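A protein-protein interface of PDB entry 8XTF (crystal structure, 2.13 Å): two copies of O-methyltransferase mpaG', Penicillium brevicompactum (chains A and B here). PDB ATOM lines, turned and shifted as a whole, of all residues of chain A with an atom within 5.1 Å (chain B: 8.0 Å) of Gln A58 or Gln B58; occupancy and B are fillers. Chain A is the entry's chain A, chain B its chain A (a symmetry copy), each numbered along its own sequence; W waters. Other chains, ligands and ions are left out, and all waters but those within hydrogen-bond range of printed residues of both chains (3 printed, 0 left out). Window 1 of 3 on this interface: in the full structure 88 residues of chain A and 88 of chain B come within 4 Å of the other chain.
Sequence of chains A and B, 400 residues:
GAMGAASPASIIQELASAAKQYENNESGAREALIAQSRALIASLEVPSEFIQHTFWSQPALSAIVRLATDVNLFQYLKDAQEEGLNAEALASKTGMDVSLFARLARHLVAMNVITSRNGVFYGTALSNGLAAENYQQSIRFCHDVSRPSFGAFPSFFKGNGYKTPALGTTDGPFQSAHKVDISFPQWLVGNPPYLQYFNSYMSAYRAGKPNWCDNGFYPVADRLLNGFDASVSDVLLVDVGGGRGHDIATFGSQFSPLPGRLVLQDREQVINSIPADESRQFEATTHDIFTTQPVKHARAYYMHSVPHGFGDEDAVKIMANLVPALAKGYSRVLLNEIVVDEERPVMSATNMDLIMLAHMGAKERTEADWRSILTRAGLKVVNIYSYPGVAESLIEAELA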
ATOM      1  N   GLN A  52      36.491  18.669 -16.540  1.00  0.00           N
ATOM      2  CA  GLN A  52      36.507  18.363 -15.113  1.00  0.00           C
ATOM      3  C   GLN A  52      35.113  18.026 -14.608  1.00  0.00           C
ATOM      4  O   GLN A  52      34.928  17.041 -13.890  1.00  0.00           O
ATOM      5  CB  GLN A  52      37.103  19.529 -14.318  1.00  0.00           C
ATOM      6  CG  GLN A  52      38.623  19.625 -14.483  1.00  0.00           C
ATOM      7  CD  GLN A  52      39.294  20.394 -13.378  1.00  0.00           C
ATOM      8  OE1 GLN A  52      38.740  20.535 -12.281  1.00  0.00           O
ATOM      9  NE2 GLN A  52      40.500  20.900 -13.651  1.00  0.00           N
ATOM     10  N   HIS A  53      34.111  18.811 -14.991  1.00  0.00           N
ATOM     11  CA  HIS A  53      32.766  18.542 -14.499  1.00  0.00           C
ATOM     12  C   HIS A  53      32.240  17.212 -15.043  1.00  0.00           C
ATOM     13  O   HIS A  53      31.790  16.354 -14.281  1.00  0.00           O
ATOM     14  CB  HIS A  53      31.830  19.694 -14.861  1.00  0.00           C
ATOM     15  CG  HIS A  53      30.439  19.485 -14.366  1.00  0.00           C
ATOM     16  ND1 HIS A  53      29.412  19.068 -15.184  1.00  0.00           N
ATOM     17  CD2 HIS A  53      29.913  19.588 -13.121  1.00  0.00           C
ATOM     18  CE1 HIS A  53      28.307  18.945 -14.468  1.00  0.00           C
ATOM     19  NE2 HIS A  53      28.591  19.240 -13.212  1.00  0.00           N
ATOM     20  N   THR A  54      32.328  17.011 -16.358  1.00  0.00           N
ATOM     21  CA  THR A  54      31.765  15.815 -16.976  1.00  0.00           C
ATOM     22  C   THR A  54      32.494  14.543 -16.548  1.00  0.00           C
ATOM     23  O   THR A  54      31.856  13.524 -16.271  1.00  0.00           O
ATOM     24  CB  THR A  54      31.813  15.945 -18.497  1.00  0.00           C
ATOM     25  OG1 THR A  54      31.169  17.160 -18.872  1.00  0.00           O
ATOM     26  CG2 THR A  54      31.108  14.765 -19.173  1.00  0.00           C
ATOM     27  N   TRP A  56      35.197  14.251 -14.077  1.00  0.00           N
ATOM     28  CA  TRP A  56      35.639  14.117 -12.690  1.00  0.00           C
ATOM     29  C   TRP A  56      34.490  14.295 -11.706  1.00  0.00           C
ATOM     30  O   TRP A  56      34.175  13.367 -10.959  1.00  0.00           O
ATOM     31  CB  TRP A  56      36.740  15.122 -12.330  1.00  0.00           C
ATOM     32  CG  TRP A  56      37.941  15.171 -13.220  1.00  0.00           C
ATOM     33  CD1 TRP A  56      38.188  14.430 -14.353  1.00  0.00           C
ATOM     34  CD2 TRP A  56      39.072  16.031 -13.048  1.00  0.00           C
ATOM     35  NE1 TRP A  56      39.407  14.782 -14.883  1.00  0.00           N
ATOM     36  CE2 TRP A  56      39.969  15.759 -14.099  1.00  0.00           C
ATOM     37  CE3 TRP A  56      39.419  16.998 -12.090  1.00  0.00           C
ATOM     38  CZ2 TRP A  56      41.182  16.419 -14.227  1.00  0.00           C
ATOM     39  CZ3 TRP A  56      40.625  17.642 -12.212  1.00  0.00           C
ATOM     40  CH2 TRP A  56      41.489  17.359 -13.279  1.00  0.00           C
ATOM     41  N   SER A  57      33.874  15.482 -11.672  1.00  0.00           N
ATOM     42  CA  SER A  57      32.872  15.788 -10.659  1.00  0.00           C
ATOM     43  C   SER A  57      31.712  14.807 -10.702  1.00  0.00           C
ATOM     44  O   SER A  57      31.272  14.309  -9.664  1.00  0.00           O
ATOM     45  CB  SER A  57      32.343  17.211 -10.829  1.00  0.00           C
ATOM     46  OG  SER A  57      33.409  18.123 -10.958  1.00  0.00           O
ATOM     47  N   GLN A  58      31.184  14.543 -11.893  1.00  0.00           N
ATOM     48  CA  GLN A  58      29.954  13.760 -11.983  1.00  0.00           C
ATOM     49  C   GLN A  58      30.198  12.276 -11.716  1.00  0.00           C
ATOM     50  O   GLN A  58      29.440  11.680 -10.928  1.00  0.00           O
ATOM     51  CB  GLN A  58      29.289  14.014 -13.336  1.00  0.00           C
ATOM     52  CG  GLN A  58      28.593  15.365 -13.437  1.00  0.00           C
ATOM     53  CD  GLN A  58      27.405  15.425 -12.495  1.00  0.00           C
ATOM     54  OE1 GLN A  58      26.799  14.402 -12.196  1.00  0.00           O
ATOM     55  NE2 GLN A  58      27.078  16.611 -12.015  1.00  0.00           N
ATOM     56  N   PRO A  59      31.206  11.620 -12.310  1.00  0.00           N
ATOM     57  CA  PRO A  59      31.471  10.230 -11.911  1.00  0.00           C
ATOM     58  C   PRO A  59      31.784  10.092 -10.436  1.00  0.00           C
ATOM     59  O   PRO A  59      31.350   9.120  -9.812  1.00  0.00           O
ATOM     60  CB  PRO A  59      32.669   9.835 -12.786  1.00  0.00           C
ATOM     61  CG  PRO A  59      32.565  10.715 -13.971  1.00  0.00           C
ATOM     62  CD  PRO A  59      32.057  12.019 -13.447  1.00  0.00           C
ATOM     63  N   ALA A  60      32.528  11.037  -9.861  1.00  0.00           N
ATOM     64  CA  ALA A  60      32.761  11.003  -8.423  1.00  0.00           C
ATOM     65  C   ALA A  60      31.455  11.175  -7.654  1.00  0.00           C
ATOM     66  O   ALA A  60      31.208  10.464  -6.676  1.00  0.00           O
ATOM     67  CB  ALA A  60      33.769  12.078  -8.024  1.00  0.00           C
ATOM     68  N   LEU A  61      30.592  12.085  -8.109  1.00  0.00           N
ATOM     69  CA  LEU A  61      29.320  12.332  -7.438  1.00  0.00           C
ATOM     70  C   LEU A  61      28.430  11.098  -7.458  1.00  0.00           C
ATOM     71  O   LEU A  61      27.823  10.736  -6.441  1.00  0.00           O
ATOM     72  CB  LEU A  61      28.606  13.502  -8.108  1.00  0.00           C
ATOM     73  CG  LEU A  61      27.198  13.791  -7.587  1.00  0.00           C
ATOM     74  CD1 LEU A  61      27.280  14.162  -6.139  1.00  0.00           C
ATOM     75  CD2 LEU A  61      26.559  14.929  -8.404  1.00  0.00           C
ATOM     76  N   SER A  62      28.309  10.463  -8.625  1.00  0.00           N
ATOM     77  CA  SER A  62      27.531   9.235  -8.727  1.00  0.00           C
ATOM     78  C   SER A  62      28.056   8.172  -7.780  1.00  0.00           C
ATOM     79  O   SER A  62      27.271   7.467  -7.135  1.00  0.00           O
ATOM     80  CB  SER A  62      27.561   8.706 -10.154  1.00  0.00           C
ATOM     81  OG  SER A  62      26.703   9.479 -10.948  1.00  0.00           O
ATOM     82  N   ALA A  63      29.382   8.038  -7.694  1.00  0.00           N
ATOM     83  CA  ALA A  63      29.974   6.999  -6.854  1.00  0.00           C
ATOM     84  C   ALA A  63      29.724   7.272  -5.374  1.00  0.00           C
ATOM     85  O   ALA A  63      29.408   6.356  -4.615  1.00  0.00           O
ATOM     86  CB  ALA A  63      31.475   6.894  -7.124  1.00  0.00           C
ATOM     87  N   MET A 111      29.106  19.808  -4.567  1.00  0.00           N
ATOM     88  CA  MET A 111      28.091  19.540  -5.578  1.00  0.00           C
ATOM     89  C   MET A 111      26.686  19.925  -5.124  1.00  0.00           C
ATOM     90  O   MET A 111      25.718  19.569  -5.799  1.00  0.00           O
ATOM     91  CB  MET A 111      28.109  18.061  -5.975  1.00  0.00           C
ATOM     92  CG  MET A 111      29.462  17.578  -6.518  1.00  0.00           C
ATOM     93  SD  MET A 111      30.028  18.519  -7.952  1.00  0.00           S
ATOM     94  CE  MET A 111      28.900  17.870  -9.179  1.00  0.00           C
ATOM     95  N   ARG B  38      24.887  26.773 -10.572  1.00  0.00           N
ATOM     96  CA  ARG B  38      24.744  25.405 -10.098  1.00  0.00           C
ATOM     97  C   ARG B  38      23.978  25.370  -8.791  1.00  0.00           C
ATOM     98  O   ARG B  38      23.166  24.468  -8.566  1.00  0.00           O
ATOM     99  CB  ARG B  38      26.109  24.756  -9.930  1.00  0.00           C
ATOM    100  CG  ARG B  38      26.948  24.830 -11.164  1.00  0.00           C
ATOM    101  CD  ARG B  38      27.940  23.700 -11.176  1.00  0.00           C
ATOM    102  NE  ARG B  38      28.062  23.127 -12.507  1.00  0.00           N
ATOM    103  CZ  ARG B  38      29.156  23.235 -13.248  1.00  0.00           C
ATOM    104  NH1 ARG B  38      30.228  23.877 -12.801  1.00  0.00           N
ATOM    105  NH2 ARG B  38      29.179  22.678 -14.457  1.00  0.00           N
ATOM    106  N   PHE B  50      17.267  15.272 -10.102  1.00  0.00           N
ATOM    107  CA  PHE B  50      18.649  15.023  -9.710  1.00  0.00           C
ATOM    108  C   PHE B  50      19.076  13.618 -10.113  1.00  0.00           C
ATOM    109  O   PHE B  50      20.175  13.428 -10.639  1.00  0.00           O
ATOM    110  CB  PHE B  50      18.836  15.218  -8.200  1.00  0.00           C
ATOM    111  CG  PHE B  50      20.189  14.773  -7.697  1.00  0.00           C
ATOM    112  CD1 PHE B  50      21.292  15.611  -7.800  1.00  0.00           C
ATOM    113  CD2 PHE B  50      20.364  13.511  -7.136  1.00  0.00           C
ATOM    114  CE1 PHE B  50      22.551  15.206  -7.342  1.00  0.00           C
ATOM    115  CE2 PHE B  50      21.619  13.099  -6.678  1.00  0.00           C
ATOM    116  CZ  PHE B  50      22.713  13.957  -6.773  1.00  0.00           C
ATOM    117  N   ILE B  51      18.219  12.621  -9.890  1.00  0.00           N
ATOM    118  CA  ILE B  51      18.556  11.252 -10.302  1.00  0.00           C
ATOM    119  C   ILE B  51      18.766  11.181 -11.811  1.00  0.00           C
ATOM    120  O   ILE B  51      19.748  10.602 -12.286  1.00  0.00           O
ATOM    121  CB  ILE B  51      17.465  10.262  -9.845  1.00  0.00           C
ATOM    122  CG1 ILE B  51      17.413  10.160  -8.316  1.00  0.00           C
ATOM    123  CG2 ILE B  51      17.690   8.886 -10.479  1.00  0.00           C
ATOM    124  CD1 ILE B  51      18.703   9.601  -7.700  1.00  0.00           C
ATOM    125  N   GLN B  52      17.840  11.753 -12.590  1.00  0.00           N
ATOM    126  CA  GLN B  52      17.957  11.685 -14.043  1.00  0.00           C
ATOM    127  C   GLN B  52      19.229  12.367 -14.525  1.00  0.00           C
ATOM    128  O   GLN B  52      19.961  11.816 -15.349  1.00  0.00           O
ATOM    129  CB  GLN B  52      16.726  12.304 -14.713  1.00  0.00           C
ATOM    130  CG  GLN B  52      15.494  11.400 -14.603  1.00  0.00           C
ATOM    131  CD  GLN B  52      14.440  11.706 -15.633  1.00  0.00           C
ATOM    132  OE1 GLN B  52      14.734  12.299 -16.679  1.00  0.00           O
ATOM    133  NE2 GLN B  52      13.197  11.302 -15.354  1.00  0.00           N
ATOM    134  N   HIS B  53      19.529  13.551 -14.003  1.00  0.00           N
ATOM    135  CA  HIS B  53      20.722  14.252 -14.463  1.00  0.00           C
ATOM    136  C   HIS B  53      21.991  13.495 -14.067  1.00  0.00           C
ATOM    137  O   HIS B  53      22.845  13.214 -14.908  1.00  0.00           O
ATOM    138  CB  HIS B  53      20.739  15.680 -13.921  1.00  0.00           C
ATOM    139  CG  HIS B  53      21.928  16.456 -14.376  1.00  0.00           C
ATOM    140  ND1 HIS B  53      23.024  16.680 -13.572  1.00  0.00           N
ATOM    141  CD2 HIS B  53      22.217  17.021 -15.573  1.00  0.00           C
ATOM    142  CE1 HIS B  53      23.927  17.371 -14.247  1.00  0.00           C
ATOM    143  NE2 HIS B  53      23.465  17.574 -15.469  1.00  0.00           N
ATOM    144  N   THR B  54      22.106  13.121 -12.793  1.00  0.00           N
ATOM    145  CA  THR B  54      23.323  12.482 -12.304  1.00  0.00           C
ATOM    146  C   THR B  54      23.538  11.101 -12.918  1.00  0.00           C
ATOM    147  O   THR B  54      24.662  10.754 -13.291  1.00  0.00           O
ATOM    148  CB  THR B  54      23.271  12.362 -10.782  1.00  0.00           C
ATOM    149  OG1 THR B  54      23.023  13.653 -10.230  1.00  0.00           O
ATOM    150  CG2 THR B  54      24.591  11.817 -10.226  1.00  0.00           C
ATOM    151  N   PHE B  55      22.483  10.292 -13.014  1.00  0.00           N
ATOM    152  CA  PHE B  55      22.623   8.895 -13.393  1.00  0.00           C
ATOM    153  C   PHE B  55      22.200   8.577 -14.823  1.00  0.00           C
ATOM    154  O   PHE B  55      22.510   7.483 -15.305  1.00  0.00           O
ATOM    155  CB  PHE B  55      21.829   8.018 -12.418  1.00  0.00           C
ATOM    156  CG  PHE B  55      22.402   8.003 -11.030  1.00  0.00           C
ATOM    157  CD1 PHE B  55      23.464   7.170 -10.712  1.00  0.00           C
ATOM    158  CD2 PHE B  55      21.891   8.843 -10.046  1.00  0.00           C
ATOM    159  CE1 PHE B  55      23.998   7.165  -9.433  1.00  0.00           C
ATOM    160  CE2 PHE B  55      22.411   8.848  -8.778  1.00  0.00           C
ATOM    161  CZ  PHE B  55      23.474   8.010  -8.465  1.00  0.00           C
ATOM    162  N   TRP B  56      21.514   9.483 -15.523  1.00  0.00           N
ATOM    163  CA  TRP B  56      21.194   9.274 -16.934  1.00  0.00           C
ATOM    164  C   TRP B  56      21.931  10.256 -17.837  1.00  0.00           C
ATOM    165  O   TRP B  56      22.727   9.835 -18.679  1.00  0.00           O
ATOM    166  CB  TRP B  56      19.692   9.398 -17.215  1.00  0.00           C
ATOM    167  CG  TRP B  56      18.769   8.569 -16.379  1.00  0.00           C
ATOM    168  CD1 TRP B  56      19.093   7.704 -15.359  1.00  0.00           C
ATOM    169  CD2 TRP B  56      17.342   8.539 -16.493  1.00  0.00           C
ATOM    170  NE1 TRP B  56      17.949   7.142 -14.844  1.00  0.00           N
ATOM    171  CE2 TRP B  56      16.864   7.635 -15.525  1.00  0.00           C
ATOM    172  CE3 TRP B  56      16.423   9.182 -17.338  1.00  0.00           C
ATOM    173  CZ2 TRP B  56      15.513   7.362 -15.370  1.00  0.00           C
ATOM    174  CZ3 TRP B  56      15.087   8.901 -17.190  1.00  0.00           C
ATOM    175  CH2 TRP B  56      14.642   8.009 -16.206  1.00  0.00           C
ATOM    176  N   SER B  57      21.660  11.559 -17.695  1.00  0.00           N
ATOM    177  CA  SER B  57      22.201  12.549 -18.617  1.00  0.00           C
ATOM    178  C   SER B  57      23.721  12.521 -18.645  1.00  0.00           C
ATOM    179  O   SER B  57      24.329  12.544 -19.717  1.00  0.00           O
ATOM    180  CB  SER B  57      21.724  13.953 -18.249  1.00  0.00           C
ATOM    181  OG  SER B  57      20.330  13.967 -18.055  1.00  0.00           O
ATOM    182  N   GLN B  58      24.350  12.503 -17.474  1.00  0.00           N
ATOM    183  CA  GLN B  58      25.801  12.665 -17.428  1.00  0.00           C
ATOM    184  C   GLN B  58      26.532  11.405 -17.888  1.00  0.00           C
ATOM    185  O   GLN B  58      27.461  11.523 -18.710  1.00  0.00           O
ATOM    186  CB  GLN B  58      26.217  13.110 -16.025  1.00  0.00           C
ATOM    187  CG  GLN B  58      25.913  14.572 -15.727  1.00  0.00           C
ATOM    188  CD  GLN B  58      26.753  15.482 -16.601  1.00  0.00           C
ATOM    189  OE1 GLN B  58      27.854  15.115 -16.998  1.00  0.00           O
ATOM    190  NE2 GLN B  58      26.240  16.657 -16.915  1.00  0.00           N
ATOM    191  N   PRO B  59      26.189  10.194 -17.426  1.00  0.00           N
ATOM    192  CA  PRO B  59      26.840   9.010 -18.005  1.00  0.00           C
ATOM    193  C   PRO B  59      26.619   8.891 -19.497  1.00  0.00           C
ATOM    194  O   PRO B  59      27.540   8.495 -20.217  1.00  0.00           O
ATOM    195  CB  PRO B  59      26.198   7.845 -17.240  1.00  0.00           C
ATOM    196  CG  PRO B  59      25.778   8.438 -15.950  1.00  0.00           C
ATOM    197  CD  PRO B  59      25.328   9.824 -16.286  1.00  0.00           C
ATOM    198  N   ALA B  60      25.423   9.219 -19.983  1.00  0.00           N
ATOM    199  CA  ALA B  60      25.199   9.225 -21.424  1.00  0.00           C
ATOM    200  C   ALA B  60      26.070  10.275 -22.106  1.00  0.00           C
ATOM    201  O   ALA B  60      26.665  10.006 -23.154  1.00  0.00           O
ATOM    202  CB  ALA B  60      23.722   9.465 -21.730  1.00  0.00           C
ATOM    203  N   LEU B  61      26.187  11.459 -21.504  1.00  0.00           N
ATOM    204  CA  LEU B  61      26.989  12.532 -22.083  1.00  0.00           C
ATOM    205  C   LEU B  61      28.458  12.143 -22.176  1.00  0.00           C
ATOM    206  O   LEU B  61      29.111  12.372 -23.203  1.00  0.00           O
ATOM    207  CB  LEU B  61      26.838  13.795 -21.241  1.00  0.00           C
ATOM    208  CG  LEU B  61      27.725  14.968 -21.660  1.00  0.00           C
ATOM    209  CD1 LEU B  61      27.364  15.381 -23.054  1.00  0.00           C
ATOM    210  CD2 LEU B  61      27.542  16.142 -20.680  1.00  0.00           C
ATOM    211  N   SER B  62      29.002  11.586 -21.093  1.00  0.00           N
ATOM    212  CA  SER B  62      30.383  11.120 -21.111  1.00  0.00           C
ATOM    213  C   SER B  62      30.603  10.093 -22.205  1.00  0.00           C
ATOM    214  O   SER B  62      31.626  10.125 -22.897  1.00  0.00           O
ATOM    215  CB  SER B  62      30.756  10.518 -19.763  1.00  0.00           C
ATOM    216  OG  SER B  62      30.970  11.553 -18.842  1.00  0.00           O
ATOM    217  N   ALA B  63      29.654   9.166 -22.365  1.00  0.00           N
ATOM    218  CA  ALA B  63      29.810   8.101 -23.353  1.00  0.00           C
ATOM    219  C   ALA B  63      29.768   8.652 -24.774  1.00  0.00           C
ATOM    220  O   ALA B  63      30.556   8.241 -25.628  1.00  0.00           O
ATOM    221  CB  ALA B  63      28.724   7.043 -23.165  1.00  0.00           C
ATOM    222  N   ILE B  64      28.848   9.566 -25.052  1.00  0.00           N
ATOM    223  CA  ILE B  64      28.755  10.110 -26.400  1.00  0.00           C
ATOM    224  C   ILE B  64      29.981  10.949 -26.726  1.00  0.00           C
ATOM    225  O   ILE B  64      30.532  10.870 -27.832  1.00  0.00           O
ATOM    226  CB  ILE B  64      27.460  10.913 -26.555  1.00  0.00           C
ATOM    227  CG1 ILE B  64      26.262   9.975 -26.453  1.00  0.00           C
ATOM    228  CG2 ILE B  64      27.470  11.686 -27.876  1.00  0.00           C
ATOM    229  CD1 ILE B  64      24.946  10.716 -26.237  1.00  0.00           C
ATOM    230  N   VAL B  65      30.421  11.772 -25.779  1.00  0.00           N
ATOM    231  CA  VAL B  65      31.627  12.561 -25.996  1.00  0.00           C
ATOM    232  C   VAL B  65      32.810  11.636 -26.282  1.00  0.00           C
ATOM    233  O   VAL B  65      33.597  11.883 -27.202  1.00  0.00           O
ATOM    234  CB  VAL B  65      31.876  13.476 -24.786  1.00  0.00           C
ATOM    235  CG1 VAL B  65      33.281  14.035 -24.807  1.00  0.00           C
ATOM    236  CG2 VAL B  65      30.851  14.596 -24.766  1.00  0.00           C
ATOM    237  N   HIS B 107      21.208  14.391 -27.972  1.00  0.00           N
ATOM    238  CA  HIS B 107      21.562  14.504 -26.562  1.00  0.00           C
ATOM    239  C   HIS B 107      22.668  15.532 -26.347  1.00  0.00           C
ATOM    240  O   HIS B 107      22.651  16.268 -25.357  1.00  0.00           O
ATOM    241  CB  HIS B 107      21.972  13.147 -25.994  1.00  0.00           C
ATOM    242  CG  HIS B 107      22.121  13.165 -24.507  1.00  0.00           C
ATOM    243  ND1 HIS B 107      21.093  13.535 -23.669  1.00  0.00           N
ATOM    244  CD2 HIS B 107      23.188  12.912 -23.710  1.00  0.00           C
ATOM    245  CE1 HIS B 107      21.511  13.483 -22.416  1.00  0.00           C
ATOM    246  NE2 HIS B 107      22.783  13.116 -22.414  1.00  0.00           N
ATOM    247  N   MET B 111      22.327  18.760 -23.991  1.00  0.00           N
ATOM    248  CA  MET B 111      23.326  19.067 -22.977  1.00  0.00           C
ATOM    249  C   MET B 111      24.155  20.303 -23.317  1.00  0.00           C
ATOM    250  O   MET B 111      25.161  20.556 -22.649  1.00  0.00           O
ATOM    251  CB  MET B 111      24.261  17.872 -22.768  1.00  0.00           C
ATOM    252  CG  MET B 111      23.539  16.583 -22.348  1.00  0.00           C
ATOM    253  SD  MET B 111      22.572  16.770 -20.835  1.00  0.00           S
ATOM    254  CE  MET B 111      23.909  16.829 -19.650  1.00  0.00           C
ATOM    255  N   HIS B 143      37.603   8.593 -19.891  1.00  0.00           N
ATOM    256  CA  HIS B 143      36.551   7.599 -20.009  1.00  0.00           C
ATOM    257  C   HIS B 143      37.086   6.183 -19.895  1.00  0.00           C
ATOM    258  O   HIS B 143      36.389   5.310 -19.366  1.00  0.00           O
ATOM    259  CB  HIS B 143      35.808   7.761 -21.327  1.00  0.00           C
ATOM    260  CG  HIS B 143      34.457   7.123 -21.326  1.00  0.00           C
ATOM    261  ND1 HIS B 143      34.225   5.865 -21.835  1.00  0.00           N
ATOM    262  CD2 HIS B 143      33.271   7.561 -20.843  1.00  0.00           C
ATOM    263  CE1 HIS B 143      32.948   5.558 -21.685  1.00  0.00           C
ATOM    264  NE2 HIS B 143      32.345   6.573 -21.088  1.00  0.00           N
ATOM    265  N   PHE B 150      36.415   5.512 -10.585  1.00  0.00           N
ATOM    266  CA  PHE B 150      35.278   6.042  -9.833  1.00  0.00           C
ATOM    267  C   PHE B 150      34.173   5.005  -9.698  1.00  0.00           C
ATOM    268  O   PHE B 150      33.557   4.877  -8.635  1.00  0.00           O
ATOM    269  CB  PHE B 150      34.742   7.297 -10.501  1.00  0.00           C
ATOM    270  CG  PHE B 150      35.622   8.479 -10.310  1.00  0.00           C
ATOM    271  CD1 PHE B 150      35.959   8.905  -9.035  1.00  0.00           C
ATOM    272  CD2 PHE B 150      36.153   9.142 -11.405  1.00  0.00           C
ATOM    273  CE1 PHE B 150      36.794  10.010  -8.863  1.00  0.00           C
ATOM    274  CE2 PHE B 150      36.975  10.238 -11.251  1.00  0.00           C
ATOM    275  CZ  PHE B 150      37.305  10.671  -9.983  1.00  0.00           C
ATOM    276  N   MET B 347      34.355  22.867  -5.614  1.00  0.00           N
ATOM    277  CA  MET B 347      34.471  21.829  -6.632  1.00  0.00           C
ATOM    278  C   MET B 347      35.893  21.695  -7.143  1.00  0.00           C
ATOM    279  O   MET B 347      36.382  20.581  -7.319  1.00  0.00           O
ATOM    280  CB  MET B 347      33.538  22.134  -7.804  1.00  0.00           C
ATOM    281  CG  MET B 347      32.786  20.946  -8.338  1.00  0.00           C
ATOM    282  SD  MET B 347      31.672  21.307  -9.750  1.00  0.00           S
ATOM    283  CE  MET B 347      32.799  21.106 -11.160  1.00  0.00           C
ATOM    284  N   ASN B 351      37.220  17.972  -6.667  1.00  0.00           N
ATOM    285  CA  ASN B 351      37.516  17.313  -7.939  1.00  0.00           C
ATOM    286  C   ASN B 351      38.890  16.674  -7.937  1.00  0.00           C
ATOM    287  O   ASN B 351      39.041  15.468  -8.167  1.00  0.00           O
ATOM    288  CB  ASN B 351      37.494  18.335  -9.079  1.00  0.00           C
ATOM    289  CG  ASN B 351      36.127  18.608  -9.573  1.00  0.00           C
ATOM    290  OD1 ASN B 351      35.162  18.011  -9.094  1.00  0.00           O
ATOM    291  ND2 ASN B 351      36.016  19.536 -10.534  1.00  0.00           N
HETATM  292  O   HOH W   1      29.285  21.221 -17.452  1.00  0.00           O
HETATM  293  O   HOH W   2      29.568  12.831 -16.850  1.00  0.00           O
HETATM  294  O   HOH W   3      26.899  11.589 -12.702  1.00  0.00           O
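The side-chain amide nitrogen of Asn B351 is in hydrogen-bond range of the side-chain amide oxygen of Gln A52, at 3.4 Å.
The backbone carbonyl oxygen (O) of Thr A54 sits close to the side-chain hydroxyl (OG) of Ser B62, 3.4 Å away.
OG of Ser A57 is in hydrogen-bond range of OD1 of Asn B351.
O of Thr B54 lies close to OG of Ser A62 (3.4 Å).
SD of Met A111 sits close to SD of Met B347, 3.7 Å away.
The backbone carbonyl oxygen (O) of Gln A52 is in hydrogen-bond range of the backbone NH (N) of Ser A57 (2.9 Å).
The backbone carbonyl oxygen (O) of His A53 is in hydrogen-bond range of the backbone NH (N) of Gln A58 (3.1 Å).
O of Phe B50 is in hydrogen-bond range of OG1 of Thr B54 (2.9 Å).
The backbone NH of Gln B58 lies within hydrogen-bond range of the backbone carbonyl oxygen of His B53, 3.1 Å away.
The backbone carbonyl oxygen (O) of Met B347 sits close to the side-chain amide oxygen (OD1) of Asn B351, at 3.4 Å.
Among the printed residues, pairs that only touch across the chains: His A53 with Arg B38, His A53 with Gln B58, His A53 with Met B347, Thr A54 with Gln B58, Trp A56 with Asn B351, Ser A57 with Met B347, Gln A58 with His B53, Gln A58 with Thr B54, Gln A58 with Gln B58, Pro A59 with Phe B150, Ala A60 with Phe B150, Ser A62 with Phe B55 and Ala A63 with Phe B150.
Gln A58 touches three residues of chain B.
Of the printed residues of chain A, Gln B58 touches His A53, Thr A54 and Gln A58.
Of the printed residues of chain B, His A53 touches Arg B38 (3.4 Å), Gln B58 (3.9 Å) and Met B347 (3.8 Å).
Of the printed residues of chain B, Gln A52 touches Asn B351 (3.4 Å).
Of the printed residues of chain B, Thr A54 touches Gln B58 (3.9 Å) and Ser B62 (3.2 Å).
Of the printed residues of chain A, Met B347 touches His A53 (3.8 Å), Ser A57 (3.1 Å) and Met A111 (3.7 Å).
Of the printed residues of chain B, Met A111 touches Met B347.
Phe B50 touches none of the printed residues of chain A.
Ile B64 touches none of the printed residues of chain A.
The nearest residue of chain B that does not touch Gln A58 is Asn B351 (6.0 Å).
His A53 touches Gln B58, and with the chains exchanged Gln A58 touches His B53.
Thr A54 touches Gln B58, and with the chains exchanged Gln A58 touches Thr B54.
Thr A54 touches Ser B62, and with the chains exchanged Ser A62 touches Thr B54.
Gln A58 touches its own counterpart, Gln B58.
Of the 18 pairs that touch across the chains among the printed residues, 7 have their exchanged pair printed and touching as well.
Water W2 lies within hydrogen-bond range of the backbone carbonyl oxygen (O) of Thr A54 (2.5 Å), the side-chain hydroxyl (OG) of Ser B62 (2.8 Å) and the side-chain amide oxygen (OE1) of Gln B58 (2.9 Å).
Water W3 lies within hydrogen-bond range of the backbone carbonyl oxygen of Thr B54, the side-chain hydroxyl of Ser A62 and the side-chain amide oxygen of Gln A58.
Water W1 bridges ND1 of His A53 (3.1 Å) and NH2 of Arg B38 (3.3 Å).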
